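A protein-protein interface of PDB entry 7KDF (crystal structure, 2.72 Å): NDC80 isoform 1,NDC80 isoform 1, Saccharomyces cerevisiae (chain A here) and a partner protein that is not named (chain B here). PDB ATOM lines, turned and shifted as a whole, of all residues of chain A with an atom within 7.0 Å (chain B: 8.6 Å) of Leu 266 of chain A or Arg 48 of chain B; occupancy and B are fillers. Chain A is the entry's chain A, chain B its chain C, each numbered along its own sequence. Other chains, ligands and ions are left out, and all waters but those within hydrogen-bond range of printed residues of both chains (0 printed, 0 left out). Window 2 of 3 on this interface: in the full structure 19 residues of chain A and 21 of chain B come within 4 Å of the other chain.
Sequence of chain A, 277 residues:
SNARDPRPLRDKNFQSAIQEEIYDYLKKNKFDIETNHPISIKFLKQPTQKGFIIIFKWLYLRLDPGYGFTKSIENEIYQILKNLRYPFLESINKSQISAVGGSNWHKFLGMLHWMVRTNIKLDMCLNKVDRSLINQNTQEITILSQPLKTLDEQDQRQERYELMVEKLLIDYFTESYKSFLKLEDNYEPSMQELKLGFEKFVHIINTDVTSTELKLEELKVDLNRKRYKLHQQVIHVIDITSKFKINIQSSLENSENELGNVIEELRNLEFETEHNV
O of Ile 41 of chain B sits at hydrogen-bond distance from OG of Ser 45 of chain B.
The guanidinium group (NH2) of Arg 48 of chain B sits at hydrogen-bond distance from the backbone carbonyl oxygen (O) of Glu 44 of chain B, 3.1 Å away.
Hydrophobic or aromatic side chains of chain A within 4 Å of the printed part of chain B: Val 262, Ile 263 and Leu 266.
Hydrophobic or aromatic side chains of chain B within 4 Å of the printed part of chain A: Val 40 and Ile 41.
Among the printed residues, 9 pairs touch across the chains.
Among the printed residues, Asp or Glu carboxylates within 4 Å of a Lys or Arg side-chain nitrogen of the other chain: Arg 267 of chain A with Glu 44 of chain B.
Of the printed residues of chain B, Leu 266 of chain A touches Glu 44, Ser 45 and Arg 48.
Of the printed residues of chain A, Val 40 of chain B touches Ile 263 and Arg 267.
Printed residues of chain B within 4 Å of Val 262 of chain A: Ile 41.
Of the printed residues of chain A, Glu 44 of chain B touches Leu 266 (3.996 Å) and Arg 267 (2.8 Å).
Printed residues of chain A within 4 Å of Ile 41 of chain B: Val 262 and Ile 263.
Printed residues of chain B within 4 Å of Arg 267 of chain A: Val 40 and Glu 44.
Glu 265 of chain A touches none of the printed residues of chain B.
The nearest residue of chain A that does not touch Arg 48 of chain B is Leu 269 of chain A (4.4 Å).
The nearest printed residue of chain A that does not touch Asp 37 of chain B is Val 262 of chain A (7.1 Å).
Among the printed residues, merely in contact across the chains: Leu 266 of chain A with Ser 45 of chain B, Arg 267 of chain A with Val 40 of chain B, Ile 263 of chain A with Ile 41 of chain B, Ile 263 of chain A with Val 40 of chain B, Ile 263 of chain A with Asp 37 of chain B, Val 262 of chain A with Ile 41 of chain B and Leu 266 of chain A with Glu 44 of chain B.
The backbone carbonyl oxygen (O) of Leu 266 of chain A is in hydrogen-bond range of the guanidinium group (NH2) of Arg 48 of chain B, at 3.1 Å.
OE2 of Glu 44 of chain B lies within salt-bridge range of NH2 of Arg 267 of chain A, 2.8 Å away.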
ATOM      1  N   ASN A 261      18.221 -30.133  -5.256  1.00  0.00           N
ATOM      2  CA  ASN A 261      18.502 -29.123  -4.242  1.00  0.00           C
ATOM      3  C   ASN A 261      18.607 -27.734  -4.860  1.00  0.00           C
ATOM      4  O   ASN A 261      18.207 -26.741  -4.240  1.00  0.00           O
ATOM      5  CB  ASN A 261      19.779 -29.481  -3.490  1.00  0.00           C
ATOM      6  CG  ASN A 261      19.654 -30.783  -2.728  1.00  0.00           C
ATOM      7  OD1 ASN A 261      18.552 -31.200  -2.377  1.00  0.00           O
ATOM      8  ND2 ASN A 261      20.784 -31.431  -2.463  1.00  0.00           N
ATOM      9  N   VAL A 262      19.147 -27.643  -6.078  1.00  0.00           N
ATOM     10  CA  VAL A 262      19.189 -26.357  -6.766  1.00  0.00           C
ATOM     11  C   VAL A 262      17.774 -25.852  -7.020  1.00  0.00           C
ATOM     12  O   VAL A 262      17.468 -24.674  -6.803  1.00  0.00           O
ATOM     13  CB  VAL A 262      19.992 -26.476  -8.074  1.00  0.00           C
ATOM     14  CG1 VAL A 262      19.921 -25.177  -8.872  1.00  0.00           C
ATOM     15  CG2 VAL A 262      21.431 -26.854  -7.775  1.00  0.00           C
ATOM     16  N   ILE A 263      16.885 -26.744  -7.459  1.00  0.00           N
ATOM     17  CA  ILE A 263      15.525 -26.344  -7.797  1.00  0.00           C
ATOM     18  C   ILE A 263      14.763 -25.899  -6.551  1.00  0.00           C
ATOM     19  O   ILE A 263      13.942 -24.976  -6.612  1.00  0.00           O
ATOM     20  CB  ILE A 263      14.817 -27.490  -8.545  1.00  0.00           C
ATOM     21  CG1 ILE A 263      15.465 -27.683  -9.916  1.00  0.00           C
ATOM     22  CG2 ILE A 263      13.336 -27.203  -8.713  1.00  0.00           C
ATOM     23  CD1 ILE A 263      14.899 -28.828 -10.708  1.00  0.00           C
ATOM     24  N   GLU A 264      15.024 -26.532  -5.401  1.00  0.00           N
ATOM     25  CA  GLU A 264      14.412 -26.058  -4.161  1.00  0.00           C
ATOM     26  C   GLU A 264      14.829 -24.627  -3.847  1.00  0.00           C
ATOM     27  O   GLU A 264      13.993 -23.798  -3.463  1.00  0.00           O
ATOM     28  CB  GLU A 264      14.772 -26.971  -2.990  1.00  0.00           C
ATOM     29  CG  GLU A 264      13.707 -27.995  -2.639  1.00  0.00           C
ATOM     30  CD  GLU A 264      14.117 -28.887  -1.481  1.00  0.00           C
ATOM     31  OE1 GLU A 264      15.060 -28.515  -0.750  1.00  0.00           O
ATOM     32  OE2 GLU A 264      13.505 -29.964  -1.304  1.00  0.00           O
ATOM     33  N   GLU A 265      16.121 -24.318  -4.000  1.00  0.00           N
ATOM     34  CA  GLU A 265      16.595 -22.963  -3.732  1.00  0.00           C
ATOM     35  C   GLU A 265      15.966 -21.955  -4.687  1.00  0.00           C
ATOM     36  O   GLU A 265      15.534 -20.876  -4.263  1.00  0.00           O
ATOM     37  CB  GLU A 265      18.121 -22.918  -3.818  1.00  0.00           C
ATOM     38  CG  GLU A 265      18.812 -23.634  -2.668  1.00  0.00           C
ATOM     39  CD  GLU A 265      20.289 -23.872  -2.922  1.00  0.00           C
ATOM     40  OE1 GLU A 265      20.727 -23.740  -4.086  1.00  0.00           O
ATOM     41  OE2 GLU A 265      21.011 -24.188  -1.952  1.00  0.00           O
ATOM     42  N   LEU A 266      15.893 -22.294  -5.977  1.00  0.00           N
ATOM     43  CA  LEU A 266      15.216 -21.429  -6.939  1.00  0.00           C
ATOM     44  C   LEU A 266      13.759 -21.187  -6.572  1.00  0.00           C
ATOM     45  O   LEU A 266      13.210 -20.127  -6.891  1.00  0.00           O
ATOM     46  CB  LEU A 266      15.310 -22.023  -8.344  1.00  0.00           C
ATOM     47  CG  LEU A 266      16.529 -21.719  -9.214  1.00  0.00           C
ATOM     48  CD1 LEU A 266      16.564 -20.232  -9.534  1.00  0.00           C
ATOM     49  CD2 LEU A 266      17.801 -22.114  -8.513  1.00  0.00           C
ATOM     50  N   ARG A 267      13.115 -22.151  -5.918  1.00  0.00           N
ATOM     51  CA  ARG A 267      11.705 -22.034  -5.580  1.00  0.00           C
ATOM     52  C   ARG A 267      11.454 -21.640  -4.130  1.00  0.00           C
ATOM     53  O   ARG A 267      10.292 -21.503  -3.735  1.00  0.00           O
ATOM     54  CB  ARG A 267      10.982 -23.347  -5.890  1.00  0.00           C
ATOM     55  CG  ARG A 267      10.982 -23.696  -7.360  1.00  0.00           C
ATOM     56  CD  ARG A 267      10.296 -25.020  -7.614  1.00  0.00           C
ATOM     57  NE  ARG A 267      10.179 -25.290  -9.042  1.00  0.00           N
ATOM     58  CZ  ARG A 267       9.946 -26.491  -9.553  1.00  0.00           C
ATOM     59  NH1 ARG A 267       9.805 -27.537  -8.748  1.00  0.00           N
ATOM     60  NH2 ARG A 267       9.863 -26.647 -10.868  1.00  0.00           N
ATOM     61  N   ASN A 268      12.501 -21.452  -3.329  1.00  0.00           N
ATOM     62  CA  ASN A 268      12.331 -21.070  -1.927  1.00  0.00           C
ATOM     63  C   ASN A 268      12.237 -19.551  -1.867  1.00  0.00           C
ATOM     64  O   ASN A 268      13.241 -18.839  -1.807  1.00  0.00           O
ATOM     65  CB  ASN A 268      13.470 -21.610  -1.073  1.00  0.00           C
ATOM     66  CG  ASN A 268      13.312 -21.264   0.397  1.00  0.00           C
ATOM     67  OD1 ASN A 268      12.302 -20.690   0.814  1.00  0.00           O
ATOM     68  ND2 ASN A 268      14.309 -21.626   1.196  1.00  0.00           N
ATOM     69  N   LEU A 269      11.003 -19.051  -1.874  1.00  0.00           N
ATOM     70  CA  LEU A 269      10.729 -17.621  -1.883  1.00  0.00           C
ATOM     71  C   LEU A 269      10.322 -17.092  -0.513  1.00  0.00           C
ATOM     72  O   LEU A 269       9.835 -15.962  -0.417  1.00  0.00           O
ATOM     73  CB  LEU A 269       9.645 -17.308  -2.914  1.00  0.00           C
ATOM     74  CG  LEU A 269       9.900 -17.881  -4.309  1.00  0.00           C
ATOM     75  CD1 LEU A 269       8.762 -17.524  -5.250  1.00  0.00           C
ATOM     76  CD2 LEU A 269      11.234 -17.388  -4.856  1.00  0.00           C
ATOM     77  N   ASP B  37      15.422 -31.555 -15.369  1.00  0.00           N
ATOM     78  CA  ASP B  37      15.805 -30.681 -14.267  1.00  0.00           C
ATOM     79  C   ASP B  37      16.663 -29.524 -14.755  1.00  0.00           C
ATOM     80  O   ASP B  37      16.528 -28.395 -14.269  1.00  0.00           O
ATOM     81  CB  ASP B  37      16.529 -31.486 -13.186  1.00  0.00           C
ATOM     82  CG  ASP B  37      15.623 -32.515 -12.517  1.00  0.00           C
ATOM     83  OD1 ASP B  37      14.385 -32.415 -12.682  1.00  0.00           O
ATOM     84  OD2 ASP B  37      16.143 -33.429 -11.835  1.00  0.00           O
ATOM     85  N   VAL B  40      14.426 -27.003 -16.197  1.00  0.00           N
ATOM     86  CA  VAL B  40      13.719 -26.305 -15.129  1.00  0.00           C
ATOM     87  C   VAL B  40      14.619 -25.246 -14.502  1.00  0.00           C
ATOM     88  O   VAL B  40      14.198 -24.105 -14.268  1.00  0.00           O
ATOM     89  CB  VAL B  40      13.212 -27.312 -14.082  1.00  0.00           C
ATOM     90  CG1 VAL B  40      12.874 -26.604 -12.775  1.00  0.00           C
ATOM     91  CG2 VAL B  40      12.018 -28.088 -14.630  1.00  0.00           C
ATOM     92  N   ILE B  41      15.875 -25.606 -14.221  1.00  0.00           N
ATOM     93  CA  ILE B  41      16.805 -24.629 -13.660  1.00  0.00           C
ATOM     94  C   ILE B  41      17.014 -23.483 -14.638  1.00  0.00           C
ATOM     95  O   ILE B  41      16.982 -22.308 -14.256  1.00  0.00           O
ATOM     96  CB  ILE B  41      18.139 -25.297 -13.282  1.00  0.00           C
ATOM     97  CG1 ILE B  41      17.930 -26.333 -12.177  1.00  0.00           C
ATOM     98  CG2 ILE B  41      19.151 -24.247 -12.844  1.00  0.00           C
ATOM     99  CD1 ILE B  41      19.044 -27.356 -12.089  1.00  0.00           C
ATOM    100  N   LYS B  42      17.205 -23.804 -15.920  1.00  0.00           N
ATOM    101  CA  LYS B  42      17.426 -22.765 -16.919  1.00  0.00           C
ATOM    102  C   LYS B  42      16.223 -21.833 -17.027  1.00  0.00           C
ATOM    103  O   LYS B  42      16.367 -20.607 -16.945  1.00  0.00           O
ATOM    104  CB  LYS B  42      17.739 -23.405 -18.272  1.00  0.00           C
ATOM    105  CG  LYS B  42      17.651 -22.457 -19.452  1.00  0.00           C
ATOM    106  CD  LYS B  42      18.442 -23.000 -20.635  1.00  0.00           C
ATOM    107  CE  LYS B  42      18.337 -22.092 -21.852  1.00  0.00           C
ATOM    108  NZ  LYS B  42      18.027 -22.862 -23.089  1.00  0.00           N
ATOM    109  N   GLU B  43      15.020 -22.396 -17.185  1.00  0.00           N
ATOM    110  CA  GLU B  43      13.847 -21.558 -17.428  1.00  0.00           C
ATOM    111  C   GLU B  43      13.469 -20.748 -16.193  1.00  0.00           C
ATOM    112  O   GLU B  43      13.055 -19.590 -16.311  1.00  0.00           O
ATOM    113  CB  GLU B  43      12.665 -22.408 -17.907  1.00  0.00           C
ATOM    114  CG  GLU B  43      11.976 -23.244 -16.838  1.00  0.00           C
ATOM    115  CD  GLU B  43      11.102 -24.345 -17.420  1.00  0.00           C
ATOM    116  OE1 GLU B  43      10.428 -25.049 -16.634  1.00  0.00           O
ATOM    117  OE2 GLU B  43      11.090 -24.511 -18.660  1.00  0.00           O
ATOM    118  N   GLU B  44      13.612 -21.329 -15.001  1.00  0.00           N
ATOM    119  CA  GLU B  44      13.221 -20.632 -13.783  1.00  0.00           C
ATOM    120  C   GLU B  44      14.309 -19.713 -13.245  1.00  0.00           C
ATOM    121  O   GLU B  44      14.031 -18.925 -12.334  1.00  0.00           O
ATOM    122  CB  GLU B  44      12.818 -21.638 -12.705  1.00  0.00           C
ATOM    123  CG  GLU B  44      11.531 -22.383 -13.012  1.00  0.00           C
ATOM    124  CD  GLU B  44      10.995 -23.125 -11.811  1.00  0.00           C
ATOM    125  OE1 GLU B  44      11.342 -22.741 -10.673  1.00  0.00           O
ATOM    126  OE2 GLU B  44      10.226 -24.092 -12.002  1.00  0.00           O
ATOM    127  N   SER B  45      15.531 -19.798 -13.773  1.00  0.00           N
ATOM    128  CA  SER B  45      16.590 -18.859 -13.432  1.00  0.00           C
ATOM    129  C   SER B  45      16.692 -17.701 -14.412  1.00  0.00           C
ATOM    130  O   SER B  45      17.353 -16.705 -14.098  1.00  0.00           O
ATOM    131  CB  SER B  45      17.949 -19.568 -13.371  1.00  0.00           C
ATOM    132  OG  SER B  45      17.921 -20.664 -12.478  1.00  0.00           O
ATOM    133  N   GLU B  46      16.050 -17.806 -15.579  1.00  0.00           N
ATOM    134  CA  GLU B  46      16.335 -16.880 -16.672  1.00  0.00           C
ATOM    135  C   GLU B  46      16.023 -15.439 -16.290  1.00  0.00           C
ATOM    136  O   GLU B  46      16.876 -14.555 -16.426  1.00  0.00           O
ATOM    137  CB  GLU B  46      15.551 -17.283 -17.920  1.00  0.00           C
ATOM    138  CG  GLU B  46      15.918 -16.474 -19.151  1.00  0.00           C
ATOM    139  CD  GLU B  46      14.799 -16.416 -20.171  1.00  0.00           C
ATOM    140  OE1 GLU B  46      13.722 -16.990 -19.907  1.00  0.00           O
ATOM    141  OE2 GLU B  46      14.997 -15.792 -21.236  1.00  0.00           O
ATOM    142  N   ALA B  47      14.806 -15.184 -15.800  1.00  0.00           N
ATOM    143  CA  ALA B  47      14.384 -13.807 -15.551  1.00  0.00           C
ATOM    144  C   ALA B  47      15.243 -13.145 -14.481  1.00  0.00           C
ATOM    145  O   ALA B  47      15.643 -11.984 -14.629  1.00  0.00           O
ATOM    146  CB  ALA B  47      12.907 -13.766 -15.156  1.00  0.00           C
ATOM    147  N   ARG B  48      15.537 -13.866 -13.398  1.00  0.00           N
ATOM    148  CA  ARG B  48      16.416 -13.308 -12.376  1.00  0.00           C
ATOM    149  C   ARG B  48      17.808 -13.047 -12.938  1.00  0.00           C
ATOM    150  O   ARG B  48      18.404 -11.998 -12.673  1.00  0.00           O
ATOM    151  CB  ARG B  48      16.480 -14.242 -11.166  1.00  0.00           C
ATOM    152  CG  ARG B  48      15.446 -13.929 -10.083  1.00  0.00           C
ATOM    153  CD  ARG B  48      15.412 -15.011  -9.014  1.00  0.00           C
ATOM    154  NE  ARG B  48      14.775 -16.228  -9.509  1.00  0.00           N
ATOM    155  CZ  ARG B  48      14.470 -17.277  -8.753  1.00  0.00           C
ATOM    156  NH1 ARG B  48      14.743 -17.265  -7.455  1.00  0.00           N
ATOM    157  NH2 ARG B  48      13.891 -18.339  -9.296  1.00  0.00           N
ATOM    158  N   LEU B  49      18.322 -13.972 -13.755  1.00  0.00           N
ATOM    159  CA  LEU B  49      19.699 -13.871 -14.230  1.00  0.00           C
ATOM    160  C   LEU B  49      19.903 -12.672 -15.148  1.00  0.00           C
ATOM    161  O   LEU B  49      21.006 -12.114 -15.199  1.00  0.00           O
ATOM    162  CB  LEU B  49      20.105 -15.169 -14.931  1.00  0.00           C
ATOM    163  CG  LEU B  49      20.587 -16.274 -13.984  1.00  0.00           C
ATOM    164  CD1 LEU B  49      21.124 -17.462 -14.761  1.00  0.00           C
ATOM    165  CD2 LEU B  49      21.646 -15.730 -13.039  1.00  0.00           C
ATOM    166  N   LYS B  50      18.861 -12.253 -15.869  1.00  0.00           N
ATOM    167  CA  LYS B  50      18.970 -11.070 -16.711  1.00  0.00           C
ATOM    168  C   LYS B  50      18.921  -9.790 -15.893  1.00  0.00           C
ATOM    169  O   LYS B  50      19.596  -8.813 -16.237  1.00  0.00           O
ATOM    170  CB  LYS B  50      17.854 -11.064 -17.752  1.00  0.00           C
ATOM    171  CG  LYS B  50      18.026  -9.978 -18.776  1.00  0.00           C
ATOM    172  CD  LYS B  50      16.918  -9.960 -19.798  1.00  0.00           C
ATOM    173  CE  LYS B  50      17.082 -11.193 -20.673  1.00  0.00           C
ATOM    174  NZ  LYS B  50      16.228 -11.174 -21.896  1.00  0.00           N
ATOM    175  N   LEU B  51      18.126  -9.770 -14.822  1.00  0.00           N
ATOM    176  CA  LEU B  51      18.142  -8.622 -13.922  1.00  0.00           C
ATOM    177  C   LEU B  51      19.528  -8.434 -13.323  1.00  0.00           C
ATOM    178  O   LEU B  51      20.060  -7.320 -13.295  1.00  0.00           O
ATOM    179  CB  LEU B  51      17.087  -8.788 -12.828  1.00  0.00           C
ATOM    180  CG  LEU B  51      15.635  -8.585 -13.261  1.00  0.00           C
ATOM    181  CD1 LEU B  51      14.679  -9.067 -12.181  1.00  0.00           C
ATOM    182  CD2 LEU B  51      15.392  -7.120 -13.584  1.00  0.00           C
ATOM    183  N   TYR B  52      20.139  -9.524 -12.859  1.00  0.00           N
ATOM    184  CA  TYR B  52      21.523  -9.447 -12.411  1.00  0.00           C
ATOM    185  C   TYR B  52      22.465  -9.127 -13.565  1.00  0.00           C
ATOM    186  O   TYR B  52      23.539  -8.556 -13.348  1.00  0.00           O
ATOM    187  CB  TYR B  52      21.939 -10.755 -11.744  1.00  0.00           C
ATOM    188  CG  TYR B  52      21.149 -11.144 -10.511  1.00  0.00           C
ATOM    189  CD1 TYR B  52      21.220 -10.388  -9.350  1.00  0.00           C
ATOM    190  CD2 TYR B  52      20.378 -12.300 -10.492  1.00  0.00           C
ATOM    191  CE1 TYR B  52      20.508 -10.746  -8.216  1.00  0.00           C
ATOM    192  CE2 TYR B  52      19.666 -12.669  -9.363  1.00  0.00           C
ATOM    193  CZ  TYR B  52      19.736 -11.890  -8.228  1.00  0.00           C
ATOM    194  OH  TYR B  52      19.031 -12.251  -7.101  1.00  0.00           O
ATOM    195  N   ARG B  53      22.090  -9.499 -14.793  1.00  0.00           N
ATOM    196  CA  ARG B  53      22.925  -9.185 -15.947  1.00  0.00           C
ATOM    197  C   ARG B  53      22.876  -7.698 -16.279  1.00  0.00           C
ATOM    198  O   ARG B  53      23.898  -7.104 -16.639  1.00  0.00           O
ATOM    199  CB  ARG B  53      22.491 -10.018 -17.153  1.00  0.00           C
ATOM    200  CG  ARG B  53      23.406  -9.885 -18.357  1.00  0.00           C
ATOM    201  CD  ARG B  53      22.987 -10.810 -19.485  1.00  0.00           C
ATOM    202  NE  ARG B  53      22.017 -10.179 -20.375  1.00  0.00           N
ATOM    203  CZ  ARG B  53      21.309 -10.832 -21.290  1.00  0.00           C
ATOM    204  NH1 ARG B  53      21.463 -12.140 -21.438  1.00  0.00           N
ATOM    205  NH2 ARG B  53      20.448 -10.177 -22.057  1.00  0.00           N
ATOM    206  N   SER B  54      21.697  -7.080 -16.165  1.00  0.00           N
ATOM    207  CA  SER B  54      21.575  -5.655 -16.452  1.00  0.00           C
ATOM    208  C   SER B  54      22.346  -4.801 -15.455  1.00  0.00           C
ATOM    209  O   SER B  54      22.620  -3.631 -15.740  1.00  0.00           O
ATOM    210  CB  SER B  54      20.102  -5.237 -16.474  1.00  0.00           C
ATOM    211  OG  SER B  54      19.444  -5.582 -15.268  1.00  0.00           O
ATOM    212  N   LEU B  55      22.701  -5.361 -14.295  1.00  0.00           N
ATOM    213  CA  LEU B  55      23.576  -4.666 -13.360  1.00  0.00           C
ATOM    214  C   LEU B  55      24.985  -4.497 -13.907  1.00  0.00           C
ATOM    215  O   LEU B  55      25.755  -3.695 -13.368  1.00  0.00           O
ATOM    216  CB  LEU B  55      23.636  -5.420 -12.033  1.00  0.00           C
ATOM    217  CG  LEU B  55      22.582  -5.071 -10.986  1.00  0.00           C
ATOM    218  CD1 LEU B  55      22.584  -6.103  -9.869  1.00  0.00           C
ATOM    219  CD2 LEU B  55      22.853  -3.684 -10.435  1.00  0.00           C
